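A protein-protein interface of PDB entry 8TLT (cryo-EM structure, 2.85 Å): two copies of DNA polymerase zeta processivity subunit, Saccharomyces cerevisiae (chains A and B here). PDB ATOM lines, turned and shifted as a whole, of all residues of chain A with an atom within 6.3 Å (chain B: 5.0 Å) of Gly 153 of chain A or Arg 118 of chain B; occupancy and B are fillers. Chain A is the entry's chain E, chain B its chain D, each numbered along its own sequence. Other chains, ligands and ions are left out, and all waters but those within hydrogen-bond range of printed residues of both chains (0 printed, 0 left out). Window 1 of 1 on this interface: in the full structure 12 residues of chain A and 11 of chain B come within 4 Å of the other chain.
Among the printed residues, merely in contact across the chains: Leu 152 of chain A with Asp 115 of chain B, Gly 153 of chain A with Phe 114 of chain B, Gly 153 of chain A with Arg 118 of chain B, His 154 of chain A with Phe 114 of chain B, Leu 156 of chain A with Asn 41 of chain B, Ser 175 of chain A with Asn 41 of chain B, Ser 175 of chain A with Pro 43 of chain B, Ser 175 of chain A with Arg 118 of chain B, Asn 176 of chain A with Pro 43 of chain B, Trp 177 of chain A with Arg 118 of chain B, Val 178 of chain A with Leu 42 of chain B, Val 178 of chain A with Asn 122 of chain B and Lys 179 of chain A with Ser 119 of chain B.
Printed residues of chain A that touch a printed residue of chain B: Glu 151, Leu 152, Gly 153, His 154, Leu 156, Asp 157, Ser 175, Asn 176, Trp 177, Val 178 and Lys 179.
Printed residues of chain B that touch a printed residue of chain A: Asn 41, Leu 42, Pro 43, Phe 114, Asp 115, Arg 118, Ser 119 and Asn 122.
Hydrophobic or aromatic side chains of chain B that line the printed part of chain A: Leu 42, Pro 43 and Phe 114.
The side-chain amide oxygen of Asn 41 of chain B sits close to the backbone carbonyl oxygen of Gly 153 of chain A (3.0 Å).
The side-chain carboxylate (OD2) of Asp 115 of chain B lies close to the side-chain carboxylate (OE2) of Glu 151 of chain A.
The side-chain carboxylate (OD2) of Asp 115 of chain B is in hydrogen-bond range of a ring nitrogen (NE2) of His 154 of chain A, at 3.3 Å.
OD1 of Asp 157 of chain A sits close to OD1 of Asn 41 of chain B (2.9 Å).
Printed residues of chain A within 4 Å of Arg 118 of chain B: Gly 153, Ser 175 and Trp 177.
Printed residues of chain B within 4 Å of Leu 152 of chain A: Asp 115 (3.8 Å).
Printed residues of chain B within 4 Å of Trp 177 of chain A: Arg 118 (3.7 Å).
Asp 174 of chain A touches none of the printed residues of chain B.
The nearest printed residue of chain A that does not touch Arg 118 of chain B is Val 178 of chain A (4.04 Å).
The nearest printed residue of chain A that does not touch Asn 41 of chain B is His 154 of chain A (4.3 Å).
The side-chain carboxylate (OD2) of Asp 157 of chain A lies close to a ring nitrogen (ND1) of His 154 of chain A (3.4 Å).
O of Asp 174 of chain A is in hydrogen-bond range of N of Gly 153 of chain A, at 2.7 Å.
No position is printed for both chains.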
ATOM      1  N   GLU A 151     -25.613  28.632   3.686  1.00  0.00           N
ATOM      2  CA  GLU A 151     -24.699  27.565   3.309  1.00  0.00           C
ATOM      3  C   GLU A 151     -25.209  26.933   2.025  1.00  0.00           C
ATOM      4  O   GLU A 151     -26.402  26.638   1.909  1.00  0.00           O
ATOM      5  CB  GLU A 151     -24.580  26.512   4.414  1.00  0.00           C
ATOM      6  CG  GLU A 151     -23.551  25.437   4.125  1.00  0.00           C
ATOM      7  CD  GLU A 151     -22.162  25.827   4.582  1.00  0.00           C
ATOM      8  OE1 GLU A 151     -21.985  26.094   5.789  1.00  0.00           O
ATOM      9  OE2 GLU A 151     -21.248  25.872   3.734  1.00  0.00           O
ATOM     10  N   LEU A 152     -24.311  26.722   1.070  1.00  0.00           N
ATOM     11  CA  LEU A 152     -24.676  26.192  -0.233  1.00  0.00           C
ATOM     12  C   LEU A 152     -23.922  24.896  -0.500  1.00  0.00           C
ATOM     13  O   LEU A 152     -22.881  24.619   0.101  1.00  0.00           O
ATOM     14  CB  LEU A 152     -24.391  27.208  -1.344  1.00  0.00           C
ATOM     15  CG  LEU A 152     -25.173  28.517  -1.241  1.00  0.00           C
ATOM     16  CD1 LEU A 152     -24.617  29.562  -2.190  1.00  0.00           C
ATOM     17  CD2 LEU A 152     -26.651  28.288  -1.499  1.00  0.00           C
ATOM     18  N   GLY A 153     -24.467  24.102  -1.418  1.00  0.00           N
ATOM     19  CA  GLY A 153     -23.885  22.813  -1.725  1.00  0.00           C
ATOM     20  C   GLY A 153     -24.170  21.733  -0.711  1.00  0.00           C
ATOM     21  O   GLY A 153     -23.468  20.718  -0.690  1.00  0.00           O
ATOM     22  N   HIS A 154     -25.182  21.918   0.138  1.00  0.00           N
ATOM     23  CA  HIS A 154     -25.523  20.935   1.158  1.00  0.00           C
ATOM     24  C   HIS A 154     -26.985  20.507   1.107  1.00  0.00           C
ATOM     25  O   HIS A 154     -27.452  19.836   2.034  1.00  0.00           O
ATOM     26  CB  HIS A 154     -25.195  21.475   2.553  1.00  0.00           C
ATOM     27  CG  HIS A 154     -23.757  21.325   2.936  1.00  0.00           C
ATOM     28  ND1 HIS A 154     -23.298  20.280   3.709  1.00  0.00           N
ATOM     29  CD2 HIS A 154     -22.676  22.089   2.657  1.00  0.00           C
ATOM     30  CE1 HIS A 154     -21.996  20.406   3.888  1.00  0.00           C
ATOM     31  NE2 HIS A 154     -21.593  21.496   3.259  1.00  0.00           N
ATOM     32  N   LYS A 155     -27.720  20.873   0.061  1.00  0.00           N
ATOM     33  CA  LYS A 155     -29.116  20.482  -0.063  1.00  0.00           C
ATOM     34  C   LYS A 155     -29.306  19.194  -0.852  1.00  0.00           C
ATOM     35  O   LYS A 155     -30.447  18.751  -1.020  1.00  0.00           O
ATOM     36  CB  LYS A 155     -29.930  21.607  -0.710  1.00  0.00           C
ATOM     37  CG  LYS A 155     -30.265  22.743   0.238  1.00  0.00           C
ATOM     38  CD  LYS A 155     -31.326  23.657  -0.346  1.00  0.00           C
ATOM     39  CE  LYS A 155     -32.681  22.974  -0.370  1.00  0.00           C
ATOM     40  N   LEU A 156     -28.228  18.589  -1.342  1.00  0.00           N
ATOM     41  CA  LEU A 156     -28.300  17.307  -2.028  1.00  0.00           C
ATOM     42  C   LEU A 156     -27.972  16.132  -1.118  1.00  0.00           C
ATOM     43  O   LEU A 156     -27.908  14.996  -1.596  1.00  0.00           O
ATOM     44  CB  LEU A 156     -27.360  17.297  -3.237  1.00  0.00           C
ATOM     45  CG  LEU A 156     -27.868  17.920  -4.537  1.00  0.00           C
ATOM     46  CD1 LEU A 156     -26.739  18.029  -5.544  1.00  0.00           C
ATOM     47  CD2 LEU A 156     -29.018  17.114  -5.104  1.00  0.00           C
ATOM     48  N   ASP A 157     -27.759  16.374   0.175  1.00  0.00           N
ATOM     49  CA  ASP A 157     -27.460  15.300   1.112  1.00  0.00           C
ATOM     50  C   ASP A 157     -28.697  14.531   1.554  1.00  0.00           C
ATOM     51  O   ASP A 157     -28.557  13.443   2.126  1.00  0.00           O
ATOM     52  CB  ASP A 157     -26.747  15.857   2.347  1.00  0.00           C
ATOM     53  CG  ASP A 157     -25.570  16.741   1.992  1.00  0.00           C
ATOM     54  OD1 ASP A 157     -24.773  16.348   1.117  1.00  0.00           O
ATOM     55  OD2 ASP A 157     -25.438  17.826   2.595  1.00  0.00           O
ATOM     56  N   ASP A 174     -29.001  25.753  -5.353  1.00  0.00           N
ATOM     57  CA  ASP A 174     -28.367  25.518  -4.061  1.00  0.00           C
ATOM     58  C   ASP A 174     -27.000  24.859  -4.189  1.00  0.00           C
ATOM     59  O   ASP A 174     -26.189  24.965  -3.264  1.00  0.00           O
ATOM     60  CB  ASP A 174     -29.270  24.658  -3.178  1.00  0.00           C
ATOM     61  N   SER A 175     -26.723  24.185  -5.305  1.00  0.00           N
ATOM     62  CA  SER A 175     -25.471  23.456  -5.478  1.00  0.00           C
ATOM     63  C   SER A 175     -24.616  24.013  -6.607  1.00  0.00           C
ATOM     64  O   SER A 175     -23.604  23.399  -6.961  1.00  0.00           O
ATOM     65  CB  SER A 175     -25.750  21.971  -5.728  1.00  0.00           C
ATOM     66  OG  SER A 175     -26.424  21.783  -6.959  1.00  0.00           O
ATOM     67  N   ASN A 176     -24.981  25.161  -7.169  1.00  0.00           N
ATOM     68  CA  ASN A 176     -24.248  25.755  -8.277  1.00  0.00           C
ATOM     69  C   ASN A 176     -23.144  26.693  -7.814  1.00  0.00           C
ATOM     70  O   ASN A 176     -22.515  27.346  -8.651  1.00  0.00           O
ATOM     71  CB  ASN A 176     -25.204  26.513  -9.199  1.00  0.00           C
ATOM     72  CG  ASN A 176     -25.607  25.706 -10.411  1.00  0.00           C
ATOM     73  OD1 ASN A 176     -25.029  24.659 -10.691  1.00  0.00           O
ATOM     74  ND2 ASN A 176     -26.601  26.193 -11.142  1.00  0.00           N
ATOM     75  N   TRP A 177     -22.897  26.782  -6.510  1.00  0.00           N
ATOM     76  CA  TRP A 177     -21.936  27.727  -5.965  1.00  0.00           C
ATOM     77  C   TRP A 177     -20.903  26.993  -5.124  1.00  0.00           C
ATOM     78  O   TRP A 177     -21.204  25.981  -4.484  1.00  0.00           O
ATOM     79  CB  TRP A 177     -22.621  28.807  -5.120  1.00  0.00           C
ATOM     80  CG  TRP A 177     -23.667  29.570  -5.866  1.00  0.00           C
ATOM     81  CD1 TRP A 177     -24.908  29.132  -6.216  1.00  0.00           C
ATOM     82  CD2 TRP A 177     -23.550  30.900  -6.383  1.00  0.00           C
ATOM     83  NE1 TRP A 177     -25.579  30.111  -6.905  1.00  0.00           N
ATOM     84  CE2 TRP A 177     -24.764  31.206  -7.023  1.00  0.00           C
ATOM     85  CE3 TRP A 177     -22.539  31.863  -6.362  1.00  0.00           C
ATOM     86  CZ2 TRP A 177     -24.995  32.433  -7.636  1.00  0.00           C
ATOM     87  CZ3 TRP A 177     -22.770  33.078  -6.969  1.00  0.00           C
ATOM     88  CH2 TRP A 177     -23.986  33.354  -7.597  1.00  0.00           C
ATOM     89  N   VAL A 178     -19.681  27.518  -5.126  1.00  0.00           N
ATOM     90  CA  VAL A 178     -18.564  26.938  -4.391  1.00  0.00           C
ATOM     91  C   VAL A 178     -18.027  27.983  -3.425  1.00  0.00           C
ATOM     92  O   VAL A 178     -17.825  29.141  -3.804  1.00  0.00           O
ATOM     93  CB  VAL A 178     -17.453  26.444  -5.334  1.00  0.00           C
ATOM     94  CG1 VAL A 178     -17.801  25.073  -5.882  1.00  0.00           C
ATOM     95  CG2 VAL A 178     -17.240  27.430  -6.466  1.00  0.00           C
ATOM     96  N   LYS A 179     -17.807  27.571  -2.179  1.00  0.00           N
ATOM     97  CA  LYS A 179     -17.265  28.471  -1.170  1.00  0.00           C
ATOM     98  C   LYS A 179     -15.888  28.967  -1.586  1.00  0.00           C
ATOM     99  O   LYS A 179     -15.049  28.192  -2.054  1.00  0.00           O
ATOM    100  CB  LYS A 179     -17.186  27.754   0.176  1.00  0.00           C
ATOM    101  CG  LYS A 179     -16.721  28.624   1.325  1.00  0.00           C
ATOM    102  CD  LYS A 179     -17.624  28.458   2.531  1.00  0.00           C
ATOM    103  CE  LYS A 179     -17.460  29.611   3.502  1.00  0.00           C
ATOM    104  NZ  LYS A 179     -17.879  29.238   4.879  1.00  0.00           N
ATOM    105  N   PHE B  40     -18.794  15.857  -4.785  1.00  0.00           N
ATOM    106  CA  PHE B  40     -18.968  16.649  -3.568  1.00  0.00           C
ATOM    107  C   PHE B  40     -20.153  17.593  -3.724  1.00  0.00           C
ATOM    108  O   PHE B  40     -20.072  18.782  -3.415  1.00  0.00           O
ATOM    109  CB  PHE B  40     -17.699  17.430  -3.236  1.00  0.00           C
ATOM    110  CG  PHE B  40     -16.731  16.685  -2.363  1.00  0.00           C
ATOM    111  CD1 PHE B  40     -15.874  15.744  -2.902  1.00  0.00           C
ATOM    112  CD2 PHE B  40     -16.668  16.938  -1.005  1.00  0.00           C
ATOM    113  CE1 PHE B  40     -14.982  15.066  -2.104  1.00  0.00           C
ATOM    114  CE2 PHE B  40     -15.776  16.261  -0.202  1.00  0.00           C
ATOM    115  CZ  PHE B  40     -14.933  15.324  -0.752  1.00  0.00           C
ATOM    116  N   ASN B  41     -21.267  17.063  -4.227  1.00  0.00           N
ATOM    117  CA  ASN B  41     -22.470  17.836  -4.540  1.00  0.00           C
ATOM    118  C   ASN B  41     -22.219  18.858  -5.642  1.00  0.00           C
ATOM    119  O   ASN B  41     -22.991  19.808  -5.797  1.00  0.00           O
ATOM    120  CB  ASN B  41     -23.036  18.535  -3.297  1.00  0.00           C
ATOM    121  CG  ASN B  41     -23.675  17.572  -2.324  1.00  0.00           C
ATOM    122  OD1 ASN B  41     -23.613  17.764  -1.112  1.00  0.00           O
ATOM    123  ND2 ASN B  41     -24.281  16.520  -2.850  1.00  0.00           N
ATOM    124  N   LEU B  42     -21.149  18.682  -6.407  1.00  0.00           N
ATOM    125  CA  LEU B  42     -20.798  19.617  -7.461  1.00  0.00           C
ATOM    126  C   LEU B  42     -21.651  19.377  -8.705  1.00  0.00           C
ATOM    127  O   LEU B  42     -22.042  18.244  -8.990  1.00  0.00           O
ATOM    128  CB  LEU B  42     -19.320  19.485  -7.812  1.00  0.00           C
ATOM    129  CG  LEU B  42     -18.350  19.981  -6.739  1.00  0.00           C
ATOM    130  CD1 LEU B  42     -17.053  19.201  -6.779  1.00  0.00           C
ATOM    131  CD2 LEU B  42     -18.087  21.465  -6.905  1.00  0.00           C
ATOM    132  N   PRO B  43     -21.953  20.436  -9.461  1.00  0.00           N
ATOM    133  CA  PRO B  43     -22.778  20.262 -10.665  1.00  0.00           C
ATOM    134  C   PRO B  43     -22.064  19.556 -11.804  1.00  0.00           C
ATOM    135  O   PRO B  43     -22.723  19.171 -12.777  1.00  0.00           O
ATOM    136  CB  PRO B  43     -23.142  21.701 -11.049  1.00  0.00           C
ATOM    137  CG  PRO B  43     -22.035  22.526 -10.487  1.00  0.00           C
ATOM    138  CD  PRO B  43     -21.619  21.849  -9.214  1.00  0.00           C
ATOM    139  N   VAL B 113     -14.760  20.987   6.455  1.00  0.00           N
ATOM    140  CA  VAL B 113     -13.930  20.061   5.689  1.00  0.00           C
ATOM    141  C   VAL B 113     -14.590  19.731   4.356  1.00  0.00           C
ATOM    142  O   VAL B 113     -13.937  19.719   3.302  1.00  0.00           O
ATOM    143  CB  VAL B 113     -13.658  18.790   6.514  1.00  0.00           C
ATOM    144  CG1 VAL B 113     -12.932  17.757   5.679  1.00  0.00           C
ATOM    145  CG2 VAL B 113     -12.867  19.128   7.766  1.00  0.00           C
ATOM    146  N   PHE B 114     -15.897  19.460   4.383  1.00  0.00           N
ATOM    147  CA  PHE B 114     -16.621  19.149   3.156  1.00  0.00           C
ATOM    148  C   PHE B 114     -16.554  20.309   2.172  1.00  0.00           C
ATOM    149  O   PHE B 114     -16.304  20.106   0.979  1.00  0.00           O
ATOM    150  CB  PHE B 114     -18.072  18.801   3.491  1.00  0.00           C
ATOM    151  CG  PHE B 114     -18.897  18.394   2.303  1.00  0.00           C
ATOM    152  CD1 PHE B 114     -18.937  17.076   1.890  1.00  0.00           C
ATOM    153  CD2 PHE B 114     -19.650  19.328   1.611  1.00  0.00           C
ATOM    154  CE1 PHE B 114     -19.701  16.699   0.805  1.00  0.00           C
ATOM    155  CE2 PHE B 114     -20.413  18.954   0.525  1.00  0.00           C
ATOM    156  CZ  PHE B 114     -20.439  17.639   0.123  1.00  0.00           C
ATOM    157  N   ASP B 115     -16.755  21.537   2.657  1.00  0.00           N
ATOM    158  CA  ASP B 115     -16.724  22.699   1.774  1.00  0.00           C
ATOM    159  C   ASP B 115     -15.327  22.937   1.214  1.00  0.00           C
ATOM    160  O   ASP B 115     -15.179  23.276   0.033  1.00  0.00           O
ATOM    161  CB  ASP B 115     -17.221  23.937   2.516  1.00  0.00           C
ATOM    162  CG  ASP B 115     -18.731  23.989   2.608  1.00  0.00           C
ATOM    163  OD1 ASP B 115     -19.387  24.183   1.562  1.00  0.00           O
ATOM    164  OD2 ASP B 115     -19.264  23.844   3.727  1.00  0.00           O
ATOM    165  N   GLU B 116     -14.293  22.772   2.041  1.00  0.00           N
ATOM    166  CA  GLU B 116     -12.927  22.966   1.563  1.00  0.00           C
ATOM    167  C   GLU B 116     -12.580  21.960   0.474  1.00  0.00           C
ATOM    168  O   GLU B 116     -12.015  22.320  -0.568  1.00  0.00           O
ATOM    169  CB  GLU B 116     -11.945  22.860   2.727  1.00  0.00           C
ATOM    170  CG  GLU B 116     -11.914  24.084   3.622  1.00  0.00           C
ATOM    171  CD  GLU B 116     -11.580  25.353   2.865  1.00  0.00           C
ATOM    172  N   PHE B 117     -12.921  20.689   0.694  1.00  0.00           N
ATOM    173  CA  PHE B 117     -12.624  19.674  -0.311  1.00  0.00           C
ATOM    174  C   PHE B 117     -13.448  19.887  -1.574  1.00  0.00           C
ATOM    175  O   PHE B 117     -12.956  19.665  -2.685  1.00  0.00           O
ATOM    176  CB  PHE B 117     -12.852  18.280   0.268  1.00  0.00           C
ATOM    177  CG  PHE B 117     -11.755  17.824   1.187  1.00  0.00           C
ATOM    178  CD1 PHE B 117     -10.468  18.307   1.039  1.00  0.00           C
ATOM    179  CD2 PHE B 117     -12.011  16.920   2.199  1.00  0.00           C
ATOM    180  CE1 PHE B 117      -9.459  17.895   1.880  1.00  0.00           C
ATOM    181  CE2 PHE B 117     -11.002  16.503   3.043  1.00  0.00           C
ATOM    182  CZ  PHE B 117      -9.726  16.993   2.883  1.00  0.00           C
ATOM    183  N   ARG B 118     -14.700  20.328  -1.428  1.00  0.00           N
ATOM    184  CA  ARG B 118     -15.531  20.616  -2.591  1.00  0.00           C
ATOM    185  C   ARG B 118     -14.947  21.755  -3.421  1.00  0.00           C
ATOM    186  O   ARG B 118     -14.904  21.678  -4.654  1.00  0.00           O
ATOM    187  CB  ARG B 118     -16.954  20.938  -2.132  1.00  0.00           C
ATOM    188  CG  ARG B 118     -17.905  21.414  -3.213  1.00  0.00           C
ATOM    189  CD  ARG B 118     -19.179  21.967  -2.588  1.00  0.00           C
ATOM    190  NE  ARG B 118     -20.038  22.642  -3.554  1.00  0.00           N
ATOM    191  CZ  ARG B 118     -20.966  22.039  -4.284  1.00  0.00           C
ATOM    192  N   SER B 119     -14.477  22.816  -2.758  1.00  0.00           N
ATOM    193  CA  SER B 119     -13.861  23.928  -3.477  1.00  0.00           C
ATOM    194  C   SER B 119     -12.567  23.502  -4.165  1.00  0.00           C
ATOM    195  O   SER B 119     -12.309  23.886  -5.315  1.00  0.00           O
ATOM    196  CB  SER B 119     -13.605  25.091  -2.521  1.00  0.00           C
ATOM    197  N   SER B 120     -11.739  22.710  -3.477  1.00  0.00           N
ATOM    198  CA  SER B 120     -10.501  22.231  -4.088  1.00  0.00           C
ATOM    199  C   SER B 120     -10.788  21.363  -5.307  1.00  0.00           C
ATOM    200  O   SER B 120     -10.119  21.486  -6.341  1.00  0.00           O
ATOM    201  CB  SER B 120      -9.677  21.455  -3.064  1.00  0.00           C
ATOM    202  OG  SER B 120      -9.649  22.129  -1.821  1.00  0.00           O
ATOM    203  N   LEU B 121     -11.782  20.479  -5.205  1.00  0.00           N
ATOM    204  CA  LEU B 121     -12.143  19.637  -6.339  1.00  0.00           C
ATOM    205  C   LEU B 121     -12.687  20.464  -7.494  1.00  0.00           C
ATOM    206  O   LEU B 121     -12.399  20.168  -8.659  1.00  0.00           O
ATOM    207  CB  LEU B 121     -13.159  18.583  -5.904  1.00  0.00           C
ATOM    208  CG  LEU B 121     -13.001  17.195  -6.526  1.00  0.00           C
ATOM    209  CD1 LEU B 121     -11.548  16.756  -6.510  1.00  0.00           C
ATOM    210  CD2 LEU B 121     -13.869  16.197  -5.788  1.00  0.00           C
ATOM    211  N   ASN B 122     -13.485  21.494  -7.200  1.00  0.00           N
ATOM    212  CA  ASN B 122     -13.974  22.364  -8.265  1.00  0.00           C
ATOM    213  C   ASN B 122     -12.822  23.055  -8.978  1.00  0.00           C
ATOM    214  O   ASN B 122     -12.806  23.142 -10.214  1.00  0.00           O
ATOM    215  CB  ASN B 122     -14.948  23.396  -7.701  1.00  0.00           C
ATOM    216  CG  ASN B 122     -15.733  24.105  -8.786  1.00  0.00           C
